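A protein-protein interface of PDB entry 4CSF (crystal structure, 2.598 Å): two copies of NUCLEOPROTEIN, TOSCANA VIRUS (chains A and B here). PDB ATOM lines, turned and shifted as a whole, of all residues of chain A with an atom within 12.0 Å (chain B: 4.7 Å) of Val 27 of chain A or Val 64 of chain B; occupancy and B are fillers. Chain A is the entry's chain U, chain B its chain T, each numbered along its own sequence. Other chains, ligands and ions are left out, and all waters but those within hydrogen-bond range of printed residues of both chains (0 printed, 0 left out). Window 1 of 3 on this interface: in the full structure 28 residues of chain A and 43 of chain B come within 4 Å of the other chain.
O of Ser 17 of chain A sits at hydrogen-bond distance from NE1 of Trp 119 of chain B. The indole nitrogen (NE1) of Trp 26 of chain A is in hydrogen-bond range of the side-chain sulfur (SD) of Met 61 of chain B. O of Ser 17 of chain A lies within hydrogen-bond range of NZ of Lys 60 of chain B, 2.9 Å away.
Among the printed residues, merely in contact across the chains: Glu 16 of chain A with Lys 60 of chain B, Phe 30 of chain A with Leu 65 of chain B, Phe 13 of chain A with Trp 119 of chain B, Phe 30 of chain A with Met 61 of chain B, Val 27 of chain A with Ser 130 of chain B, Trp 26 of chain A with Lys 60 of chain B, Glu 16 of chain A with Trp 119 of chain B, Ile 23 of chain A with Leu 127 of chain B, Ala 18 of chain A with Trp 119 of chain B, Val 27 of chain A with Leu 127 of chain B, Val 27 of chain A with Val 64 of chain B and Ile 23 of chain A with Trp 119 of chain B.
Of the printed residues of chain B, Phe 13 of chain A touches Trp 119. Of the printed residues of chain B, Ile 23 of chain A touches Trp 119 and Leu 127. Of chain B, only Val 64, Leu 127 and Ser 130 come within 4 Å of Val 27 of chain A. Of the printed residues of chain A, Val 64 of chain B touches Val 27 (3.9 Å). Of chain A, only Phe 30 comes within 4 Å of Leu 65 of chain B. No residue of chain A comes within 4 Å of Asn 66 of chain B. Val 68 of chain B touches none of the printed residues of chain A. Of chain A, only Ile 23 and Val 27 come within 4 Å of Leu 127 of chain B. The nearest printed residue of chain A that does not touch Val 64 of chain B is Trp 26 of chain A (4.02 Å).
Printed residues of chain A that touch a printed residue of chain B: Phe 13, Glu 16, Ser 17, Ala 18, Ile 23, Trp 26, Val 27 and Phe 30. Of the 12 printed residues of chain B, 7 touch a printed residue of chain A. Hydrophobic or aromatic side chains of chain B within 4 Å of the printed part of chain A: Met 61, Val 64, Leu 65, Trp 119 and Leu 127. Among the printed residues, no Asp or Glu carboxylate lies within 4 Å of a Lys or Arg side-chain nitrogen of the other chain.
No position is printed for both chains.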
ATOM      1  N   PHE A  13       0.399   8.084  -1.187  1.00  0.00           N
ATOM      2  CA  PHE A  13       1.255   9.229  -1.476  1.00  0.00           C
ATOM      3  C   PHE A  13       1.392   9.466  -2.974  1.00  0.00           C
ATOM      4  O   PHE A  13       1.898  10.499  -3.399  1.00  0.00           O
ATOM      5  CB  PHE A  13       2.626   9.066  -0.818  1.00  0.00           C
ATOM      6  CG  PHE A  13       2.689   9.616   0.574  1.00  0.00           C
ATOM      7  CD1 PHE A  13       2.200   8.885   1.646  1.00  0.00           C
ATOM      8  CD2 PHE A  13       3.224  10.876   0.813  1.00  0.00           C
ATOM      9  CE1 PHE A  13       2.246   9.400   2.937  1.00  0.00           C
ATOM     10  CE2 PHE A  13       3.275  11.395   2.098  1.00  0.00           C
ATOM     11  CZ  PHE A  13       2.785  10.653   3.161  1.00  0.00           C
ATOM     12  N   GLU A  16      -0.903  12.100  -3.386  1.00  0.00           N
ATOM     13  CA  GLU A  16      -0.606  13.217  -2.498  1.00  0.00           C
ATOM     14  C   GLU A  16       0.057  14.339  -3.292  1.00  0.00           C
ATOM     15  O   GLU A  16       0.779  14.082  -4.256  1.00  0.00           O
ATOM     16  CB  GLU A  16       0.282  12.764  -1.340  1.00  0.00           C
ATOM     17  CG  GLU A  16       0.254  13.689  -0.131  1.00  0.00           C
ATOM     18  CD  GLU A  16      -0.921  13.447   0.801  1.00  0.00           C
ATOM     19  OE1 GLU A  16      -1.268  12.271   1.040  1.00  0.00           O
ATOM     20  OE2 GLU A  16      -1.482  14.438   1.312  1.00  0.00           O
ATOM     21  N   SER A  17      -0.195  15.582  -2.889  1.00  0.00           N
ATOM     22  CA  SER A  17       0.222  16.751  -3.668  1.00  0.00           C
ATOM     23  C   SER A  17       1.737  16.919  -3.789  1.00  0.00           C
ATOM     24  O   SER A  17       2.465  16.887  -2.795  1.00  0.00           O
ATOM     25  CB  SER A  17      -0.402  18.031  -3.095  1.00  0.00           C
ATOM     26  OG  SER A  17       0.086  18.295  -1.790  1.00  0.00           O
ATOM     27  N   ALA A  18       2.198  17.098  -5.020  1.00  0.00           N
ATOM     28  CA  ALA A  18       3.600  17.377  -5.292  1.00  0.00           C
ATOM     29  C   ALA A  18       3.726  18.748  -5.950  1.00  0.00           C
ATOM     30  O   ALA A  18       4.129  18.859  -7.111  1.00  0.00           O
ATOM     31  CB  ALA A  18       4.190  16.298  -6.198  1.00  0.00           C
ATOM     32  N   ASP A  19       3.377  19.785  -5.196  1.00  0.00           N
ATOM     33  CA  ASP A  19       3.333  21.158  -5.701  1.00  0.00           C
ATOM     34  C   ASP A  19       4.708  21.705  -6.075  1.00  0.00           C
ATOM     35  O   ASP A  19       5.609  21.794  -5.234  1.00  0.00           O
ATOM     36  CB  ASP A  19       2.687  22.075  -4.661  1.00  0.00           C
ATOM     37  CG  ASP A  19       2.242  23.392  -5.248  1.00  0.00           C
ATOM     38  OD1 ASP A  19       1.138  23.428  -5.827  1.00  0.00           O
ATOM     39  OD2 ASP A  19       2.987  24.389  -5.122  1.00  0.00           O
ATOM     40  N   SER A  20       4.844  22.084  -7.343  1.00  0.00           N
ATOM     41  CA  SER A  20       6.092  22.612  -7.897  1.00  0.00           C
ATOM     42  C   SER A  20       6.658  23.814  -7.126  1.00  0.00           C
ATOM     43  O   SER A  20       7.878  23.918  -6.918  1.00  0.00           O
ATOM     44  CB  SER A  20       5.877  22.987  -9.367  1.00  0.00           C
ATOM     45  OG  SER A  20       7.061  23.495  -9.950  1.00  0.00           O
ATOM     46  N   GLY A  21       5.766  24.713  -6.706  1.00  0.00           N
ATOM     47  CA  GLY A  21       6.149  25.920  -5.993  1.00  0.00           C
ATOM     48  C   GLY A  21       6.698  25.663  -4.604  1.00  0.00           C
ATOM     49  O   GLY A  21       7.768  26.171  -4.252  1.00  0.00           O
ATOM     50  N   THR A  22       5.969  24.878  -3.814  1.00  0.00           N
ATOM     51  CA  THR A  22       6.386  24.573  -2.446  1.00  0.00           C
ATOM     52  C   THR A  22       7.656  23.721  -2.429  1.00  0.00           C
ATOM     53  O   THR A  22       8.537  23.928  -1.592  1.00  0.00           O
ATOM     54  CB  THR A  22       5.258  23.882  -1.630  1.00  0.00           C
ATOM     55  OG1 THR A  22       5.077  22.536  -2.085  1.00  0.00           O
ATOM     56  CG2 THR A  22       3.945  24.643  -1.768  1.00  0.00           C
ATOM     57  N   ILE A  23       7.746  22.771  -3.359  1.00  0.00           N
ATOM     58  CA  ILE A  23       8.925  21.909  -3.472  1.00  0.00           C
ATOM     59  C   ILE A  23      10.189  22.719  -3.763  1.00  0.00           C
ATOM     60  O   ILE A  23      11.224  22.515  -3.126  1.00  0.00           O
ATOM     61  CB  ILE A  23       8.738  20.811  -4.548  1.00  0.00           C
ATOM     62  CG1 ILE A  23       7.776  19.730  -4.052  1.00  0.00           C
ATOM     63  CG2 ILE A  23      10.062  20.169  -4.904  1.00  0.00           C
ATOM     64  CD1 ILE A  23       7.423  18.677  -5.097  1.00  0.00           C
ATOM     65  N   ASN A  24      10.099  23.646  -4.714  1.00  0.00           N
ATOM     66  CA  ASN A  24      11.242  24.493  -5.056  1.00  0.00           C
ATOM     67  C   ASN A  24      11.665  25.425  -3.916  1.00  0.00           C
ATOM     68  O   ASN A  24      12.845  25.752  -3.776  1.00  0.00           O
ATOM     69  CB  ASN A  24      10.982  25.281  -6.347  1.00  0.00           C
ATOM     70  CG  ASN A  24      11.265  24.460  -7.603  1.00  0.00           C
ATOM     71  OD1 ASN A  24      12.243  23.706  -7.664  1.00  0.00           O
ATOM     72  ND2 ASN A  24      10.407  24.604  -8.613  1.00  0.00           N
ATOM     73  N   ALA A  25      10.700  25.841  -3.099  1.00  0.00           N
ATOM     74  CA  ALA A  25      10.996  26.646  -1.918  1.00  0.00           C
ATOM     75  C   ALA A  25      11.776  25.831  -0.877  1.00  0.00           C
ATOM     76  O   ALA A  25      12.699  26.348  -0.240  1.00  0.00           O
ATOM     77  CB  ALA A  25       9.713  27.212  -1.320  1.00  0.00           C
ATOM     78  N   TRP A  26      11.407  24.561  -0.711  1.00  0.00           N
ATOM     79  CA  TRP A  26      12.130  23.662   0.190  1.00  0.00           C
ATOM     80  C   TRP A  26      13.551  23.445  -0.309  1.00  0.00           C
ATOM     81  O   TRP A  26      14.507  23.488   0.475  1.00  0.00           O
ATOM     82  CB  TRP A  26      11.416  22.315   0.311  1.00  0.00           C
ATOM     83  CG  TRP A  26      10.122  22.384   1.062  1.00  0.00           C
ATOM     84  CD1 TRP A  26       9.746  23.336   1.963  1.00  0.00           C
ATOM     85  CD2 TRP A  26       9.024  21.462   0.969  1.00  0.00           C
ATOM     86  NE1 TRP A  26       8.485  23.062   2.439  1.00  0.00           N
ATOM     87  CE2 TRP A  26       8.022  21.922   1.845  1.00  0.00           C
ATOM     88  CE3 TRP A  26       8.797  20.298   0.232  1.00  0.00           C
ATOM     89  CZ2 TRP A  26       6.802  21.250   2.000  1.00  0.00           C
ATOM     90  CZ3 TRP A  26       7.587  19.635   0.391  1.00  0.00           C
ATOM     91  CH2 TRP A  26       6.608  20.113   1.266  1.00  0.00           C
ATOM     92  N   VAL A  27      13.678  23.211  -1.614  1.00  0.00           N
ATOM     93  CA  VAL A  27      14.982  23.054  -2.254  1.00  0.00           C
ATOM     94  C   VAL A  27      15.886  24.242  -1.946  1.00  0.00           C
ATOM     95  O   VAL A  27      17.053  24.069  -1.601  1.00  0.00           O
ATOM     96  CB  VAL A  27      14.846  22.900  -3.783  1.00  0.00           C
ATOM     97  CG1 VAL A  27      16.212  22.924  -4.454  1.00  0.00           C
ATOM     98  CG2 VAL A  27      14.108  21.611  -4.123  1.00  0.00           C
ATOM     99  N   ASN A  28      15.331  25.446  -2.059  1.00  0.00           N
ATOM    100  CA  ASN A  28      16.071  26.673  -1.774  1.00  0.00           C
ATOM    101  C   ASN A  28      16.508  26.803  -0.314  1.00  0.00           C
ATOM    102  O   ASN A  28      17.579  27.332  -0.038  1.00  0.00           O
ATOM    103  CB  ASN A  28      15.257  27.895  -2.202  1.00  0.00           C
ATOM    104  CG  ASN A  28      15.128  28.014  -3.712  1.00  0.00           C
ATOM    105  OD1 ASN A  28      15.656  27.192  -4.462  1.00  0.00           O
ATOM    106  ND2 ASN A  28      14.419  29.042  -4.165  1.00  0.00           N
ATOM    107  N   GLU A  29      15.680  26.322   0.611  1.00  0.00           N
ATOM    108  CA  GLU A  29      16.024  26.325   2.034  1.00  0.00           C
ATOM    109  C   GLU A  29      17.107  25.296   2.350  1.00  0.00           C
ATOM    110  O   GLU A  29      18.022  25.562   3.129  1.00  0.00           O
ATOM    111  CB  GLU A  29      14.789  26.014   2.883  1.00  0.00           C
ATOM    112  CG  GLU A  29      13.717  27.088   2.873  1.00  0.00           C
ATOM    113  CD  GLU A  29      12.435  26.632   3.545  1.00  0.00           C
ATOM    114  OE1 GLU A  29      12.253  25.406   3.713  1.00  0.00           O
ATOM    115  OE2 GLU A  29      11.609  27.501   3.904  1.00  0.00           O
ATOM    116  N   PHE A  30      16.983  24.120   1.734  1.00  0.00           N
ATOM    117  CA  PHE A  30      17.819  22.968   2.049  1.00  0.00           C
ATOM    118  C   PHE A  30      19.130  22.933   1.273  1.00  0.00           C
ATOM    119  O   PHE A  30      20.060  22.217   1.652  1.00  0.00           O
ATOM    120  CB  PHE A  30      17.051  21.678   1.773  1.00  0.00           C
ATOM    121  CG  PHE A  30      15.879  21.461   2.682  1.00  0.00           C
ATOM    122  CD1 PHE A  30      15.875  21.984   3.965  1.00  0.00           C
ATOM    123  CD2 PHE A  30      14.782  20.731   2.256  1.00  0.00           C
ATOM    124  CE1 PHE A  30      14.793  21.782   4.811  1.00  0.00           C
ATOM    125  CE2 PHE A  30      13.698  20.522   3.097  1.00  0.00           C
ATOM    126  CZ  PHE A  30      13.708  21.046   4.376  1.00  0.00           C
ATOM    127  N   ALA A  31      19.203  23.705   0.194  1.00  0.00           N
ATOM    128  CA  ALA A  31      20.351  23.653  -0.710  1.00  0.00           C
ATOM    129  C   ALA A  31      21.676  23.915  -0.004  1.00  0.00           C
ATOM    130  O   ALA A  31      21.717  24.554   1.050  1.00  0.00           O
ATOM    131  CB  ALA A  31      20.170  24.632  -1.855  1.00  0.00           C
ATOM    132  N   TYR A  32      22.753  23.392  -0.582  1.00  0.00           N
ATOM    133  CA  TYR A  32      24.088  23.627  -0.057  1.00  0.00           C
ATOM    134  C   TYR A  32      24.373  25.125   0.028  1.00  0.00           C
ATOM    135  O   TYR A  32      24.080  25.878  -0.903  1.00  0.00           O
ATOM    136  CB  TYR A  32      25.137  22.935  -0.931  1.00  0.00           C
ATOM    137  CG  TYR A  32      26.559  23.350  -0.606  1.00  0.00           C
ATOM    138  CD1 TYR A  32      27.251  22.779   0.458  1.00  0.00           C
ATOM    139  CD2 TYR A  32      27.206  24.315  -1.361  1.00  0.00           C
ATOM    140  CE1 TYR A  32      28.547  23.159   0.759  1.00  0.00           C
ATOM    141  CE2 TYR A  32      28.505  24.709  -1.065  1.00  0.00           C
ATOM    142  CZ  TYR A  32      29.169  24.126  -0.005  1.00  0.00           C
ATOM    143  OH  TYR A  32      30.456  24.510   0.293  1.00  0.00           O
ATOM    144  N   GLN A  33      24.928  25.556   1.153  1.00  0.00           N
ATOM    145  CA  GLN A  33      25.312  26.952   1.320  1.00  0.00           C
ATOM    146  C   GLN A  33      26.681  27.039   1.976  1.00  0.00           C
ATOM    147  O   GLN A  33      26.852  26.661   3.137  1.00  0.00           O
ATOM    148  CB  GLN A  33      24.268  27.717   2.139  1.00  0.00           C
ATOM    149  CG  GLN A  33      24.513  29.218   2.192  1.00  0.00           C
ATOM    150  CD  GLN A  33      23.485  29.955   3.030  1.00  0.00           C
ATOM    151  OE1 GLN A  33      23.745  30.308   4.184  1.00  0.00           O
ATOM    152  NE2 GLN A  33      22.308  30.196   2.452  1.00  0.00           N
ATOM    153  N   GLY A  34      27.654  27.534   1.217  1.00  0.00           N
ATOM    154  CA  GLY A  34      29.019  27.664   1.690  1.00  0.00           C
ATOM    155  C   GLY A  34      29.877  28.240   0.583  1.00  0.00           C
ATOM    156  O   GLY A  34      29.839  29.443   0.319  1.00  0.00           O
ATOM    157  N   LYS A  38      30.054  33.043  -6.895  1.00  0.00           N
ATOM    158  CA  LYS A  38      29.234  34.256  -6.958  1.00  0.00           C
ATOM    159  C   LYS A  38      29.462  35.135  -5.735  1.00  0.00           C
ATOM    160  O   LYS A  38      29.633  36.350  -5.853  1.00  0.00           O
ATOM    161  CB  LYS A  38      27.748  33.901  -7.062  1.00  0.00           C
ATOM    162  CG  LYS A  38      27.294  33.429  -8.439  1.00  0.00           C
ATOM    163  CD  LYS A  38      25.810  33.046  -8.443  1.00  0.00           C
ATOM    164  CE  LYS A  38      25.538  31.864  -7.524  1.00  0.00           C
ATOM    165  NZ  LYS A  38      24.119  31.414  -7.557  1.00  0.00           N
ATOM    166  N   ARG A 213      27.971  24.722 -10.725  1.00  0.00           N
ATOM    167  CA  ARG A 213      27.063  25.253 -11.733  1.00  0.00           C
ATOM    168  C   ARG A 213      27.233  26.759 -11.941  1.00  0.00           C
ATOM    169  O   ARG A 213      26.397  27.400 -12.575  1.00  0.00           O
ATOM    170  CB  ARG A 213      25.617  24.932 -11.352  1.00  0.00           C
ATOM    171  CG  ARG A 213      25.423  23.543 -10.765  1.00  0.00           C
ATOM    172  CD  ARG A 213      24.459  22.711 -11.593  1.00  0.00           C
ATOM    173  NE  ARG A 213      23.660  21.826 -10.749  1.00  0.00           N
ATOM    174  CZ  ARG A 213      23.924  20.538 -10.540  1.00  0.00           C
ATOM    175  NH1 ARG A 213      24.969  19.962 -11.122  1.00  0.00           N
ATOM    176  NH2 ARG A 213      23.134  19.820  -9.750  1.00  0.00           N
ATOM    177  N   LYS B  60       7.319  14.553   2.866  1.00  0.00           N
ATOM    178  CA  LYS B  60       7.674  15.256   1.640  1.00  0.00           C
ATOM    179  C   LYS B  60       8.957  16.069   1.806  1.00  0.00           C
ATOM    180  O   LYS B  60       9.856  16.018   0.956  1.00  0.00           O
ATOM    181  CB  LYS B  60       6.534  16.169   1.201  1.00  0.00           C
ATOM    182  CG  LYS B  60       5.236  15.440   0.940  1.00  0.00           C
ATOM    183  CD  LYS B  60       4.149  16.425   0.576  1.00  0.00           C
ATOM    184  CE  LYS B  60       2.842  15.714   0.354  1.00  0.00           C
ATOM    185  NZ  LYS B  60       1.741  16.647  -0.028  1.00  0.00           N
ATOM    186  N   MET B  61       9.043  16.811   2.904  1.00  0.00           N
ATOM    187  CA  MET B  61      10.232  17.618   3.167  1.00  0.00           C
ATOM    188  C   MET B  61      11.477  16.754   3.339  1.00  0.00           C
ATOM    189  O   MET B  61      12.538  17.071   2.800  1.00  0.00           O
ATOM    190  CB  MET B  61      10.026  18.521   4.382  1.00  0.00           C
ATOM    191  CG  MET B  61       8.889  19.514   4.193  1.00  0.00           C
ATOM    192  SD  MET B  61       8.959  20.932   5.301  1.00  0.00           S
ATOM    193  CE  MET B  61       8.864  20.114   6.905  1.00  0.00           C
ATOM    194  N   MET B  62      11.338  15.654   4.071  1.00  0.00           N
ATOM    195  CA  MET B  62      12.453  14.741   4.280  1.00  0.00           C
ATOM    196  C   MET B  62      12.916  14.106   2.969  1.00  0.00           C
ATOM    197  O   MET B  62      14.115  13.922   2.752  1.00  0.00           O
ATOM    198  CB  MET B  62      12.099  13.667   5.309  1.00  0.00           C
ATOM    199  CG  MET B  62      12.078  14.171   6.741  1.00  0.00           C
ATOM    200  SD  MET B  62      11.972  12.830   7.944  1.00  0.00           S
ATOM    201  CE  MET B  62      10.314  12.220   7.641  1.00  0.00           C
ATOM    202  N   ILE B  63      11.967  13.788   2.091  1.00  0.00           N
ATOM    203  CA  ILE B  63      12.306  13.240   0.781  1.00  0.00           C
ATOM    204  C   ILE B  63      13.068  14.262  -0.067  1.00  0.00           C
ATOM    205  O   ILE B  63      14.139  13.955  -0.597  1.00  0.00           O
ATOM    206  CB  ILE B  63      11.055  12.744   0.022  1.00  0.00           C
ATOM    207  CG1 ILE B  63      10.485  11.497   0.697  1.00  0.00           C
ATOM    208  CG2 ILE B  63      11.394  12.448  -1.424  1.00  0.00           C
ATOM    209  CD1 ILE B  63       9.211  10.964   0.046  1.00  0.00           C
ATOM    210  N   VAL B  64      12.518  15.474  -0.180  1.00  0.00           N
ATOM    211  CA  VAL B  64      13.168  16.547  -0.931  1.00  0.00           C
ATOM    212  C   VAL B  64      14.559  16.818  -0.364  1.00  0.00           C
ATOM    213  O   VAL B  64      15.536  16.937  -1.108  1.00  0.00           O
ATOM    214  CB  VAL B  64      12.326  17.835  -0.923  1.00  0.00           C
ATOM    215  CG1 VAL B  64      13.142  19.021  -1.416  1.00  0.00           C
ATOM    216  CG2 VAL B  64      11.060  17.651  -1.768  1.00  0.00           C
ATOM    217  N   LEU B  65      14.640  16.888   0.962  1.00  0.00           N
ATOM    218  CA  LEU B  65      15.913  17.052   1.654  1.00  0.00           C
ATOM    219  C   LEU B  65      16.888  15.940   1.277  1.00  0.00           C
ATOM    220  O   LEU B  65      18.074  16.192   1.066  1.00  0.00           O
ATOM    221  CB  LEU B  65      15.695  17.068   3.169  1.00  0.00           C
ATOM    222  CG  LEU B  65      16.935  17.299   4.039  1.00  0.00           C
ATOM    223  CD1 LEU B  65      17.562  18.648   3.731  1.00  0.00           C
ATOM    224  CD2 LEU B  65      16.596  17.189   5.515  1.00  0.00           C
ATOM    225  N   ASN B  66      16.379  14.714   1.181  1.00  0.00           N
ATOM    226  CA  ASN B  66      17.206  13.561   0.824  1.00  0.00           C
ATOM    227  C   ASN B  66      17.676  13.616  -0.629  1.00  0.00           C
ATOM    228  O   ASN B  66      18.817  13.256  -0.941  1.00  0.00           O
ATOM    229  CB  ASN B  66      16.462  12.245   1.104  1.00  0.00           C
ATOM    230  CG  ASN B  66      17.239  11.016   0.647  1.00  0.00           C
ATOM    231  OD1 ASN B  66      16.759  10.238  -0.176  1.00  0.00           O
ATOM    232  ND2 ASN B  66      18.447  10.843   1.175  1.00  0.00           N
ATOM    233  N   LEU B  67      16.796  14.080  -1.511  1.00  0.00           N
ATOM    234  CA  LEU B  67      17.118  14.168  -2.930  1.00  0.00           C
ATOM    235  C   LEU B  67      18.215  15.192  -3.227  1.00  0.00           C
ATOM    236  O   LEU B  67      19.053  14.967  -4.101  1.00  0.00           O
ATOM    237  CB  LEU B  67      15.863  14.481  -3.760  1.00  0.00           C
ATOM    238  CG  LEU B  67      14.741  13.437  -3.730  1.00  0.00           C
ATOM    239  CD1 LEU B  67      13.577  13.833  -4.630  1.00  0.00           C
ATOM    240  CD2 LEU B  67      15.287  12.082  -4.124  1.00  0.00           C
ATOM    241  N   VAL B  68      18.222  16.307  -2.499  1.00  0.00           N
ATOM    242  CA  VAL B  68      19.153  17.391  -2.813  1.00  0.00           C
ATOM    243  C   VAL B  68      20.393  17.437  -1.912  1.00  0.00           C
ATOM    244  O   VAL B  68      21.406  18.031  -2.284  1.00  0.00           O
ATOM    245  CB  VAL B  68      18.453  18.784  -2.834  1.00  0.00           C
ATOM    246  CG1 VAL B  68      17.073  18.678  -3.460  1.00  0.00           C
ATOM    247  CG2 VAL B  68      18.363  19.372  -1.448  1.00  0.00           C
ATOM    248  N   TRP B 119       5.742   8.939  -3.755  1.00  0.00           N
ATOM    249  CA  TRP B 119       5.831  10.397  -3.791  1.00  0.00           C
ATOM    250  C   TRP B 119       7.198  10.864  -4.294  1.00  0.00           C
ATOM    251  O   TRP B 119       7.287  11.833  -5.054  1.00  0.00           O
ATOM    252  CB  TRP B 119       5.521  11.023  -2.427  1.00  0.00           C
ATOM    253  CG  TRP B 119       5.306  12.512  -2.525  1.00  0.00           C
ATOM    254  CD1 TRP B 119       4.129  13.154  -2.791  1.00  0.00           C
ATOM    255  CD2 TRP B 119       6.299  13.538  -2.380  1.00  0.00           C
ATOM    256  NE1 TRP B 119       4.327  14.516  -2.809  1.00  0.00           N
ATOM    257  CE2 TRP B 119       5.650  14.779  -2.563  1.00  0.00           C
ATOM    258  CE3 TRP B 119       7.672  13.531  -2.110  1.00  0.00           C
ATOM    259  CZ2 TRP B 119       6.329  16.002  -2.483  1.00  0.00           C
ATOM    260  CZ3 TRP B 119       8.344  14.744  -2.030  1.00  0.00           C
ATOM    261  CH2 TRP B 119       7.671  15.961  -2.217  1.00  0.00           C
ATOM    262  N   LEU B 127      12.225  18.602  -9.448  1.00  0.00           N
ATOM    263  CA  LEU B 127      13.516  19.162  -9.037  1.00  0.00           C
ATOM    264  C   LEU B 127      14.738  18.499  -9.684  1.00  0.00           C
ATOM    265  O   LEU B 127      15.820  18.484  -9.096  1.00  0.00           O
ATOM    266  CB  LEU B 127      13.645  19.115  -7.505  1.00  0.00           C
ATOM    267  CG  LEU B 127      13.143  17.863  -6.773  1.00  0.00           C
ATOM    268  CD1 LEU B 127      13.888  16.602  -7.180  1.00  0.00           C
ATOM    269  CD2 LEU B 127      13.232  18.059  -5.269  1.00  0.00           C
ATOM    270  N   SER B 130      18.194  20.111  -9.653  1.00  0.00           N
ATOM    271  CA  SER B 130      18.811  20.400  -8.357  1.00  0.00           C
ATOM    272  C   SER B 130      19.457  19.152  -7.746  1.00  0.00           C
ATOM    273  O   SER B 130      19.966  19.182  -6.621  1.00  0.00           O
ATOM    274  CB  SER B 130      17.782  20.992  -7.387  1.00  0.00           C
ATOM    275  OG  SER B 130      17.227  22.195  -7.898  1.00  0.00           O
